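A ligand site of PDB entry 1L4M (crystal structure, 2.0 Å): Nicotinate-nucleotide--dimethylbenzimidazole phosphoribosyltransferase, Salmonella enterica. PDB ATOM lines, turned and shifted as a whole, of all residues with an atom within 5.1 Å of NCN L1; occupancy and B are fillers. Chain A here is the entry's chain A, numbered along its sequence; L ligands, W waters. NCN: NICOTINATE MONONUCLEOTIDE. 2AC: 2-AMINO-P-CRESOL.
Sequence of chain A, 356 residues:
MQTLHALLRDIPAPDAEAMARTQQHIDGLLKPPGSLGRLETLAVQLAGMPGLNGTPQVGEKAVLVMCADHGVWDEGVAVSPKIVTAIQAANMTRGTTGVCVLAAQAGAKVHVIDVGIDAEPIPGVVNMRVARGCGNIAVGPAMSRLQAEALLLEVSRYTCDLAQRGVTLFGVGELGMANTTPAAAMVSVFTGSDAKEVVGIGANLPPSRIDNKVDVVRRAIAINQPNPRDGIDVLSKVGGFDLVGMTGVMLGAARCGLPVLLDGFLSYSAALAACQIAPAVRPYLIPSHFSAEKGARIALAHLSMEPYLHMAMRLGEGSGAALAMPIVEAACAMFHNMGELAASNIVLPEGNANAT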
ATOM      1  N   VAL A  77      -6.004  -7.732  16.161  1.00  0.00           N
ATOM      2  CA  VAL A  77      -6.068  -8.965  16.955  1.00  0.00           C
ATOM      3  C   VAL A  77      -5.264  -8.943  18.260  1.00  0.00           C
ATOM      4  O   VAL A  77      -5.277  -9.916  19.018  1.00  0.00           O
ATOM      5  CB  VAL A  77      -5.595 -10.182  16.116  1.00  0.00           C
ATOM      6  CG1 VAL A  77      -6.508 -10.384  14.917  1.00  0.00           C
ATOM      7  CG2 VAL A  77      -4.161  -9.981  15.646  1.00  0.00           C
ATOM      8  N   ALA A  78      -4.565  -7.843  18.524  1.00  0.00           N
ATOM      9  CA  ALA A  78      -3.738  -7.700  19.744  1.00  0.00           C
ATOM     10  C   ALA A  78      -3.849  -6.303  20.368  1.00  0.00           C
ATOM     11  O   ALA A  78      -3.720  -5.294  19.693  1.00  0.00           O
ATOM     12  CB  ALA A  78      -2.267  -8.000  19.410  1.00  0.00           C
ATOM     13  N   SER A  80      -1.786  -5.215  22.829  1.00  0.00           N
ATOM     14  CA  SER A  80      -0.470  -4.737  23.245  1.00  0.00           C
ATOM     15  C   SER A  80       0.123  -3.847  22.160  1.00  0.00           C
ATOM     16  O   SER A  80       0.075  -4.203  20.976  1.00  0.00           O
ATOM     17  CB  SER A  80       0.505  -5.912  23.475  1.00  0.00           C
ATOM     18  OG  SER A  80       0.074  -6.807  24.472  1.00  0.00           O
ATOM     19  N   GLU A 174       9.479 -17.389  22.788  1.00  0.00           N
ATOM     20  CA  GLU A 174       9.256 -16.376  21.769  1.00  0.00           C
ATOM     21  C   GLU A 174       8.785 -15.069  22.374  1.00  0.00           C
ATOM     22  O   GLU A 174       8.469 -14.991  23.567  1.00  0.00           O
ATOM     23  CB  GLU A 174       8.226 -16.865  20.738  1.00  0.00           C
ATOM     24  CG  GLU A 174       6.970 -17.549  21.329  1.00  0.00           C
ATOM     25  CD  GLU A 174       6.271 -16.695  22.377  1.00  0.00           C
ATOM     26  OE1 GLU A 174       5.737 -15.624  22.036  1.00  0.00           O
ATOM     27  OE2 GLU A 174       6.267 -17.077  23.555  1.00  0.00           O
ATOM     28  N   LEU A 175       8.742 -14.043  21.534  1.00  0.00           N
ATOM     29  CA  LEU A 175       8.284 -12.712  21.903  1.00  0.00           C
ATOM     30  C   LEU A 175       7.827 -12.062  20.599  1.00  0.00           C
ATOM     31  O   LEU A 175       8.613 -11.881  19.675  1.00  0.00           O
ATOM     32  CB  LEU A 175       9.425 -11.910  22.519  1.00  0.00           C
ATOM     33  CG  LEU A 175       9.090 -10.474  22.947  1.00  0.00           C
ATOM     34  CD1 LEU A 175       7.953 -10.504  24.004  1.00  0.00           C
ATOM     35  CD2 LEU A 175      10.335  -9.795  23.530  1.00  0.00           C
ATOM     36  N   GLY A 176       6.544 -11.701  20.525  1.00  0.00           N
ATOM     37  CA  GLY A 176       6.025 -11.067  19.328  1.00  0.00           C
ATOM     38  C   GLY A 176       4.552 -10.725  19.492  1.00  0.00           C
ATOM     39  O   GLY A 176       3.711 -11.633  19.588  1.00  0.00           O
ATOM     40  N   MET A 177       4.229  -9.444  19.521  1.00  0.00           N
ATOM     41  CA  MET A 177       2.834  -9.035  19.681  1.00  0.00           C
ATOM     42  C   MET A 177       2.008  -9.594  18.524  1.00  0.00           C
ATOM     43  O   MET A 177       2.420  -9.511  17.356  1.00  0.00           O
ATOM     44  CB  MET A 177       2.713  -7.503  19.722  1.00  0.00           C
ATOM     45  CG  MET A 177       3.574  -6.847  20.809  1.00  0.00           C
ATOM     46  SD  MET A 177       3.328  -7.560  22.455  1.00  0.00           S
ATOM     47  CE  MET A 177       4.817  -8.626  22.647  1.00  0.00           C
ATOM     48  N   ALA A 178       0.865 -10.176  18.868  1.00  0.00           N
ATOM     49  CA  ALA A 178      -0.083 -10.775  17.930  1.00  0.00           C
ATOM     50  C   ALA A 178       0.272 -12.176  17.473  1.00  0.00           C
ATOM     51  O   ALA A 178      -0.456 -12.739  16.630  1.00  0.00           O
ATOM     52  CB  ALA A 178      -0.258  -9.869  16.694  1.00  0.00           C
ATOM     53  N   ASN A 179       1.341 -12.789  17.985  1.00  0.00           N
ATOM     54  CA  ASN A 179       1.677 -14.115  17.479  1.00  0.00           C
ATOM     55  C   ASN A 179       0.742 -15.279  17.846  1.00  0.00           C
ATOM     56  O   ASN A 179       0.892 -16.369  17.314  1.00  0.00           O
ATOM     57  CB  ASN A 179       3.165 -14.478  17.738  1.00  0.00           C
ATOM     58  CG  ASN A 179       3.514 -14.675  19.208  1.00  0.00           C
ATOM     59  OD1 ASN A 179       2.639 -14.720  20.074  1.00  0.00           O
ATOM     60  ND2 ASN A 179       4.814 -14.811  19.491  1.00  0.00           N
ATOM     61  N   THR A 180      -0.241 -15.058  18.720  1.00  0.00           N
ATOM     62  CA  THR A 180      -1.145 -16.173  19.011  1.00  0.00           C
ATOM     63  C   THR A 180      -2.135 -16.320  17.861  1.00  0.00           C
ATOM     64  O   THR A 180      -2.850 -17.324  17.760  1.00  0.00           O
ATOM     65  CB  THR A 180      -1.915 -16.014  20.342  1.00  0.00           C
ATOM     66  OG1 THR A 180      -2.750 -14.851  20.273  1.00  0.00           O
ATOM     67  CG2 THR A 180      -0.964 -15.865  21.510  1.00  0.00           C
ATOM     68  N   THR A 181      -2.185 -15.329  16.974  1.00  0.00           N
ATOM     69  CA  THR A 181      -3.080 -15.427  15.823  1.00  0.00           C
ATOM     70  C   THR A 181      -2.478 -16.424  14.812  1.00  0.00           C
ATOM     71  O   THR A 181      -3.113 -17.406  14.470  1.00  0.00           O
ATOM     72  CB  THR A 181      -3.337 -14.043  15.198  1.00  0.00           C
ATOM     73  OG1 THR A 181      -4.188 -13.297  16.071  1.00  0.00           O
ATOM     74  CG2 THR A 181      -4.033 -14.176  13.835  1.00  0.00           C
ATOM     75  N   ILE A 201      -7.616 -15.842  23.977  1.00  0.00           N
ATOM     76  CA  ILE A 201      -7.512 -14.422  24.315  1.00  0.00           C
ATOM     77  C   ILE A 201      -6.088 -13.857  24.242  1.00  0.00           C
ATOM     78  O   ILE A 201      -5.885 -12.664  24.424  1.00  0.00           O
ATOM     79  CB  ILE A 201      -8.125 -14.162  25.710  1.00  0.00           C
ATOM     80  N   GLY A 202      -5.102 -14.722  23.991  1.00  0.00           N
ATOM     81  CA  GLY A 202      -3.721 -14.249  23.901  1.00  0.00           C
ATOM     82  C   GLY A 202      -3.326 -13.390  25.083  1.00  0.00           C
ATOM     83  O   GLY A 202      -3.603 -13.749  26.236  1.00  0.00           O
ATOM     84  N   ALA A 203      -2.686 -12.249  24.839  1.00  0.00           N
ATOM     85  CA  ALA A 203      -2.267 -11.358  25.915  1.00  0.00           C
ATOM     86  C   ALA A 203      -3.405 -10.414  26.288  1.00  0.00           C
ATOM     87  O   ALA A 203      -3.396  -9.233  25.922  1.00  0.00           O
ATOM     88  CB  ALA A 203      -1.017 -10.550  25.492  1.00  0.00           C
ATOM     89  N   LYS A 213     -10.860 -11.866  15.735  1.00  0.00           N
ATOM     90  CA  LYS A 213      -9.671 -12.705  15.681  1.00  0.00           C
ATOM     91  C   LYS A 213      -9.992 -14.003  14.941  1.00  0.00           C
ATOM     92  O   LYS A 213      -9.202 -14.459  14.111  1.00  0.00           O
ATOM     93  CB  LYS A 213      -9.148 -12.978  17.095  1.00  0.00           C
ATOM     94  CG  LYS A 213      -7.759 -13.596  17.157  1.00  0.00           C
ATOM     95  CD  LYS A 213      -7.306 -13.718  18.608  1.00  0.00           C
ATOM     96  CE  LYS A 213      -5.956 -14.428  18.748  1.00  0.00           C
ATOM     97  NZ  LYS A 213      -5.567 -14.533  20.210  1.00  0.00           N
ATOM     98  N   ASP A 263       7.501 -24.771  25.567  1.00  0.00           N
ATOM     99  CA  ASP A 263       6.991 -23.759  26.483  1.00  0.00           C
ATOM    100  C   ASP A 263       5.466 -23.779  26.443  1.00  0.00           C
ATOM    101  O   ASP A 263       4.852 -24.757  26.855  1.00  0.00           O
ATOM    102  CB  ASP A 263       7.524 -22.351  26.107  1.00  0.00           C
ATOM    103  CG  ASP A 263       7.092 -21.254  27.106  1.00  0.00           C
ATOM    104  OD1 ASP A 263       6.918 -21.572  28.311  1.00  0.00           O
ATOM    105  OD2 ASP A 263       6.958 -20.094  26.697  1.00  0.00           O
ATOM    106  N   GLY A 264       4.851 -22.700  25.934  1.00  0.00           N
ATOM    107  CA  GLY A 264       3.398 -22.627  25.853  1.00  0.00           C
ATOM    108  C   GLY A 264       2.758 -22.832  24.486  1.00  0.00           C
ATOM    109  O   GLY A 264       3.324 -23.517  23.625  1.00  0.00           O
ATOM    110  N   PHE A 265       1.594 -22.217  24.269  1.00  0.00           N
ATOM    111  CA  PHE A 265       0.832 -22.363  23.021  1.00  0.00           C
ATOM    112  C   PHE A 265       1.623 -22.108  21.731  1.00  0.00           C
ATOM    113  O   PHE A 265       1.498 -22.856  20.764  1.00  0.00           O
ATOM    114  CB  PHE A 265      -0.411 -21.451  23.035  1.00  0.00           C
ATOM    115  CG  PHE A 265      -1.379 -21.727  21.911  1.00  0.00           C
ATOM    116  CD1 PHE A 265      -1.640 -20.778  20.935  1.00  0.00           C
ATOM    117  CD2 PHE A 265      -2.047 -22.945  21.836  1.00  0.00           C
ATOM    118  CE1 PHE A 265      -2.542 -21.029  19.889  1.00  0.00           C
ATOM    119  CE2 PHE A 265      -2.946 -23.214  20.798  1.00  0.00           C
ATOM    120  CZ  PHE A 265      -3.194 -22.247  19.833  1.00  0.00           C
ATOM    121  N   LEU A 266       2.421 -21.036  21.713  1.00  0.00           N
ATOM    122  CA  LEU A 266       3.203 -20.747  20.522  1.00  0.00           C
ATOM    123  C   LEU A 266       4.163 -21.883  20.205  1.00  0.00           C
ATOM    124  O   LEU A 266       4.315 -22.266  19.039  1.00  0.00           O
ATOM    125  CB  LEU A 266       4.010 -19.443  20.659  1.00  0.00           C
ATOM    126  CG  LEU A 266       3.318 -18.082  20.771  1.00  0.00           C
ATOM    127  CD1 LEU A 266       2.241 -17.975  19.714  1.00  0.00           C
ATOM    128  CD2 LEU A 266       2.704 -17.897  22.173  1.00  0.00           C
ATOM    129  N   HIS A 289       4.790 -27.035  30.635  1.00  0.00           N
ATOM    130  CA  HIS A 289       3.522 -26.748  31.274  1.00  0.00           C
ATOM    131  C   HIS A 289       2.332 -26.776  30.325  1.00  0.00           C
ATOM    132  O   HIS A 289       2.481 -26.883  29.105  1.00  0.00           O
ATOM    133  CB  HIS A 289       3.572 -25.380  31.970  1.00  0.00           C
ATOM    134  CG  HIS A 289       3.479 -24.205  31.036  1.00  0.00           C
ATOM    135  ND1 HIS A 289       4.425 -23.964  30.066  1.00  0.00           N
ATOM    136  CD2 HIS A 289       2.553 -23.225  30.919  1.00  0.00           C
ATOM    137  CE1 HIS A 289       4.083 -22.877  29.383  1.00  0.00           C
ATOM    138  NE2 HIS A 289       2.946 -22.412  29.880  1.00  0.00           N
ATOM    139  N   SER A 291      -0.386 -24.610  28.887  1.00  0.00           N
ATOM    140  CA  SER A 291      -0.770 -23.220  28.623  1.00  0.00           C
ATOM    141  C   SER A 291      -2.247 -22.936  28.855  1.00  0.00           C
ATOM    142  O   SER A 291      -3.113 -23.765  28.536  1.00  0.00           O
ATOM    143  CB  SER A 291      -0.405 -22.832  27.195  1.00  0.00           C
ATOM    144  OG  SER A 291      -0.875 -21.543  26.888  1.00  0.00           O
ATOM    145  N   GLU A 293      -3.950 -20.956  27.197  1.00  0.00           N
ATOM    146  CA  GLU A 293      -4.541 -20.579  25.931  1.00  0.00           C
ATOM    147  C   GLU A 293      -5.598 -21.627  25.569  1.00  0.00           C
ATOM    148  O   GLU A 293      -5.404 -22.833  25.767  1.00  0.00           O
ATOM    149  CB  GLU A 293      -3.448 -20.497  24.857  1.00  0.00           C
ATOM    150  CG  GLU A 293      -3.895 -19.943  23.514  1.00  0.00           C
ATOM    151  CD  GLU A 293      -4.060 -18.433  23.475  1.00  0.00           C
ATOM    152  OE1 GLU A 293      -4.091 -17.768  24.535  1.00  0.00           O
ATOM    153  OE2 GLU A 293      -4.171 -17.901  22.372  1.00  0.00           O
ATOM    154  N   MET A 313      -0.296 -20.719  33.168  1.00  0.00           N
ATOM    155  CA  MET A 313       0.571 -19.684  32.624  1.00  0.00           C
ATOM    156  C   MET A 313       0.325 -19.412  31.135  1.00  0.00           C
ATOM    157  O   MET A 313      -0.038 -20.320  30.382  1.00  0.00           O
ATOM    158  CB  MET A 313       2.036 -20.058  32.866  1.00  0.00           C
ATOM    159  CG  MET A 313       2.462 -19.884  34.314  1.00  0.00           C
ATOM    160  SD  MET A 313       4.021 -20.722  34.680  1.00  0.00           S
ATOM    161  CE  MET A 313       5.132 -19.944  33.485  1.00  0.00           C
ATOM    162  N   ARG A 314       0.509 -18.162  30.737  1.00  0.00           N
ATOM    163  CA  ARG A 314       0.292 -17.736  29.350  1.00  0.00           C
ATOM    164  C   ARG A 314       1.141 -16.521  29.028  1.00  0.00           C
ATOM    165  O   ARG A 314       0.739 -15.650  28.266  1.00  0.00           O
ATOM    166  CB  ARG A 314      -1.197 -17.426  29.146  1.00  0.00           C
ATOM    167  CG  ARG A 314      -1.781 -16.461  30.201  1.00  0.00           C
ATOM    168  CD  ARG A 314      -3.280 -16.247  29.985  1.00  0.00           C
ATOM    169  NE  ARG A 314      -3.921 -15.498  31.054  1.00  0.00           N
ATOM    170  CZ  ARG A 314      -3.866 -14.178  31.200  1.00  0.00           C
ATOM    171  NH1 ARG A 314      -3.195 -13.423  30.344  1.00  0.00           N
ATOM    172  NH2 ARG A 314      -4.501 -13.599  32.212  1.00  0.00           N
ATOM    173  N   LEU A 315       2.328 -16.445  29.630  1.00  0.00           N
ATOM    174  CA  LEU A 315       3.233 -15.315  29.391  1.00  0.00           C
ATOM    175  C   LEU A 315       4.062 -15.489  28.128  1.00  0.00           C
ATOM    176  O   LEU A 315       4.243 -14.543  27.349  1.00  0.00           O
ATOM    177  CB  LEU A 315       4.187 -15.132  30.582  1.00  0.00           C
ATOM    178  CG  LEU A 315       5.357 -14.154  30.381  1.00  0.00           C
ATOM    179  CD1 LEU A 315       4.844 -12.744  30.157  1.00  0.00           C
ATOM    180  CD2 LEU A 315       6.268 -14.191  31.617  1.00  0.00           C
ATOM    181  N   GLY A 316       4.577 -16.705  27.913  1.00  0.00           N
ATOM    182  CA  GLY A 316       5.418 -16.950  26.753  1.00  0.00           C
ATOM    183  C   GLY A 316       6.851 -16.717  27.180  1.00  0.00           C
ATOM    184  O   GLY A 316       7.205 -16.934  28.345  1.00  0.00           O
ATOM    185  N   GLU A 317       7.690 -16.275  26.244  1.00  0.00           N
ATOM    186  CA  GLU A 317       9.110 -15.993  26.493  1.00  0.00           C
ATOM    187  C   GLU A 317       9.955 -17.238  26.787  1.00  0.00           C
ATOM    188  O   GLU A 317      11.176 -17.145  26.849  1.00  0.00           O
ATOM    189  CB  GLU A 317       9.270 -15.048  27.676  1.00  0.00           C
ATOM    190  CG  GLU A 317       8.481 -13.758  27.577  1.00  0.00           C
ATOM    191  CD  GLU A 317       8.767 -12.839  28.733  1.00  0.00           C
ATOM    192  OE1 GLU A 317       9.693 -13.132  29.519  1.00  0.00           O
ATOM    193  OE2 GLU A 317       8.065 -11.808  28.857  1.00  0.00           O
HETATM  194  P   NCN L   1      -1.138 -11.728  21.494  1.00  0.00           P
HETATM  195  O1P NCN L   1      -1.407 -12.530  20.274  1.00  0.00           O
HETATM  196  O2P NCN L   1      -2.420 -11.314  22.121  1.00  0.00           O
HETATM  197  O3P NCN L   1      -0.293 -10.406  21.116  1.00  0.00           O
HETATM  198  O5' NCN L   1      -0.307 -12.601  22.529  1.00  0.00           O
HETATM  199  C5' NCN L   1       0.971 -13.130  22.132  1.00  0.00           C
HETATM  200  C4' NCN L   1       2.017 -12.580  23.052  1.00  0.00           C
HETATM  201  O4' NCN L   1       1.689 -12.905  24.436  1.00  0.00           O
HETATM  202  C3' NCN L   1       3.419 -13.089  22.796  1.00  0.00           C
HETATM  203  O3' NCN L   1       4.444 -12.078  22.949  1.00  0.00           O
HETATM  204  C2' NCN L   1       3.533 -14.277  23.814  1.00  0.00           C
HETATM  205  O2' NCN L   1       4.870 -14.276  24.396  1.00  0.00           O
HETATM  206  C1' NCN L   1       2.409 -14.040  24.840  1.00  0.00           C
HETATM  207  N1  NCN L   1       1.463 -15.192  25.092  1.00  0.00           N
HETATM  208  C6  NCN L   1       0.039 -14.989  25.135  1.00  0.00           C
HETATM  209  C5  NCN L   1      -0.698 -16.150  25.392  1.00  0.00           C
HETATM  210  C4  NCN L   1      -0.165 -17.465  25.598  1.00  0.00           C
HETATM  211  C3  NCN L   1       1.296 -17.516  25.533  1.00  0.00           C
HETATM  212  C2  NCN L   1       2.091 -16.402  25.275  1.00  0.00           C
HETATM  213  C7  NCN L   1       1.706 -18.968  25.775  1.00  0.00           C
HETATM  214  O7  NCN L   1       0.990 -19.916  26.001  1.00  0.00           O
HETATM  215  O8  NCN L   1       3.033 -19.042  25.707  1.00  0.00           O
HETATM  216  N   2AC L   2       5.926 -10.904  27.392  1.00  0.00           N
HETATM  217  O   2AC L   2       3.745 -11.039  25.567  1.00  0.00           O
HETATM  218  C1  2AC L   2       5.036  -9.773  27.252  1.00  0.00           C
HETATM  219  C2  2AC L   2       3.935  -9.839  26.335  1.00  0.00           C
HETATM  220  C3  2AC L   2       3.058  -8.787  26.163  1.00  0.00           C
HETATM  221  C4  2AC L   2       3.235  -7.623  26.904  1.00  0.00           C
HETATM  222  C5  2AC L   2       4.397  -7.567  27.876  1.00  0.00           C
HETATM  223  C6  2AC L   2       5.249  -8.659  27.995  1.00  0.00           C
HETATM  224  C8  2AC L   2       4.600  -6.311  28.686  1.00  0.00           C
HETATM  225  O   HOH W   1      -4.896 -11.700  21.024  1.00  0.00           O
HETATM  226  O   HOH W   2       4.598 -20.614  23.956  1.00  0.00           O
HETATM  227  O   HOH W   3       4.355 -19.954  28.025  1.00  0.00           O
HETATM  228  O   HOH W   4      -1.201  -8.358  22.605  1.00  0.00           O
HETATM  229  O   HOH W   5      -3.159 -12.036  18.236  1.00  0.00           O
HETATM  230  O   HOH W   6      -3.717  -9.049  23.001  1.00  0.00           O
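O3' of NCN L1 is in hydrogen-bond range of O of 2AC L2, at 2.9 Å.
O of Arg 314 lies close to N1 of NCN L1 (3.3 Å).
Ala 78 touches NCN L1 (CB to O3P, 3.5 Å).
CD1 of Leu 175 touches O3' of NCN L1, 3.99 Å away.
Met 177 touches NCN L1.
OD1 of Asn 179 touches C5' of NCN L1, 3.1 Å away.
Gly 202 touches NCN L1.
Gly 264 touches NCN L1.
Leu 266 touches NCN L1 (CD2 to C2, 3.5 Å).
Glu 293 touches NCN L1.
Gly 316 touches NCN L1.
Glu 317 touches NCN L1 (N to O2', 3.9 Å).
Hydrophobic or aromatic side chains within 4 Å of NCN L1: Ala 78, Leu 175, Met 177, Ala 203, Phe 265 and Leu 266.
The nearest printed residue that does not touch NCN L1 is Asp 263 (4.2 Å).
The side-chain hydroxyl (OG1) of Thr 180 lies within hydrogen-bond range of the side-chain amino group (NZ) of Lys 213, at 2.8 Å.
The side-chain carboxylate of Glu 293 is in hydrogen-bond range of the backbone NH of Gly 202 (3.3 Å).
The backbone NH of Glu 293 sits close to the side-chain hydroxyl of Ser 291 (3.1 Å).
The backbone carbonyl oxygen (O) of Glu 174 lies within hydrogen-bond range of the backbone NH (N) of Glu 317 (3.1 Å).
The side-chain amide oxygen of Asn 179 sits close to the backbone carbonyl oxygen of Gly 176 (3.3 Å).
OE1 of Glu 174 sits at hydrogen-bond distance from ND2 of Asn 179 (2.8 Å).
N of Ala 203 is in hydrogen-bond range of O2P of NCN L1.
The backbone NH (N) of Gly 176 is in hydrogen-bond range of an oxygen (O3') of NCN L1 (3.2 Å).
OE2 of Glu 317 is in hydrogen-bond range of N of 2AC L2 (2.7 Å).
OG of Ser 291 sits at hydrogen-bond distance from O7 of NCN L1, 2.6 Å away.
An oxygen (O3P) of NCN L1 is in hydrogen-bond range of the backbone NH (N) of Ala 178, 2.5 Å away.
O1P of NCN L1 is in hydrogen-bond range of OG1 of Thr 180 (2.7 Å).
O1P of NCN L1 is in hydrogen-bond range of N of Thr 180 (3.2 Å).
An oxygen (O2') of NCN L1 lies within hydrogen-bond range of the side-chain carboxylate of Glu 174.
An oxygen (O3') of NCN L1 is in hydrogen-bond range of the backbone carbonyl oxygen (O) of Gly 176 (3.5 Å).
O2' of NCN L1 sits at hydrogen-bond distance from O of Leu 315, 3.0 Å away.
N of Phe 265 is in hydrogen-bond range of O7 of NCN L1 (2.9 Å).
Water W4 bridges O3P of NCN L1 and OG of Ser 80.
Water W5 lies within hydrogen-bond range of the side-chain hydroxyl (OG1) of Thr 181 (2.7 Å), an oxygen (O1P) of NCN L1 (2.7 Å), the backbone carbonyl oxygen (O) of Val 77 (3.1 Å), the backbone carbonyl oxygen (O) of Ala 178 (3.2 Å) and the side-chain hydroxyl (OG1) of Thr 180 (3.5 Å).
Water W1 lies within hydrogen-bond range of O of Val 77 (2.7 Å), O2P of NCN L1 (2.7 Å) and NZ of Lys 213 (3.0 Å).
Water W6 bridges O2P of NCN L1 (2.8 Å) and O of Ala 203 (2.9 Å).
Water W3 lies within hydrogen-bond range of an oxygen (O8) of NCN L1 (2.8 Å), the side-chain carboxylate of Asp 263 (2.9 Å), the backbone NH of Gly 316 (3.3 Å), a ring nitrogen (NE2) of His 289 (3.4 Å) and the backbone NH of Gly 264 (3.5 Å).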
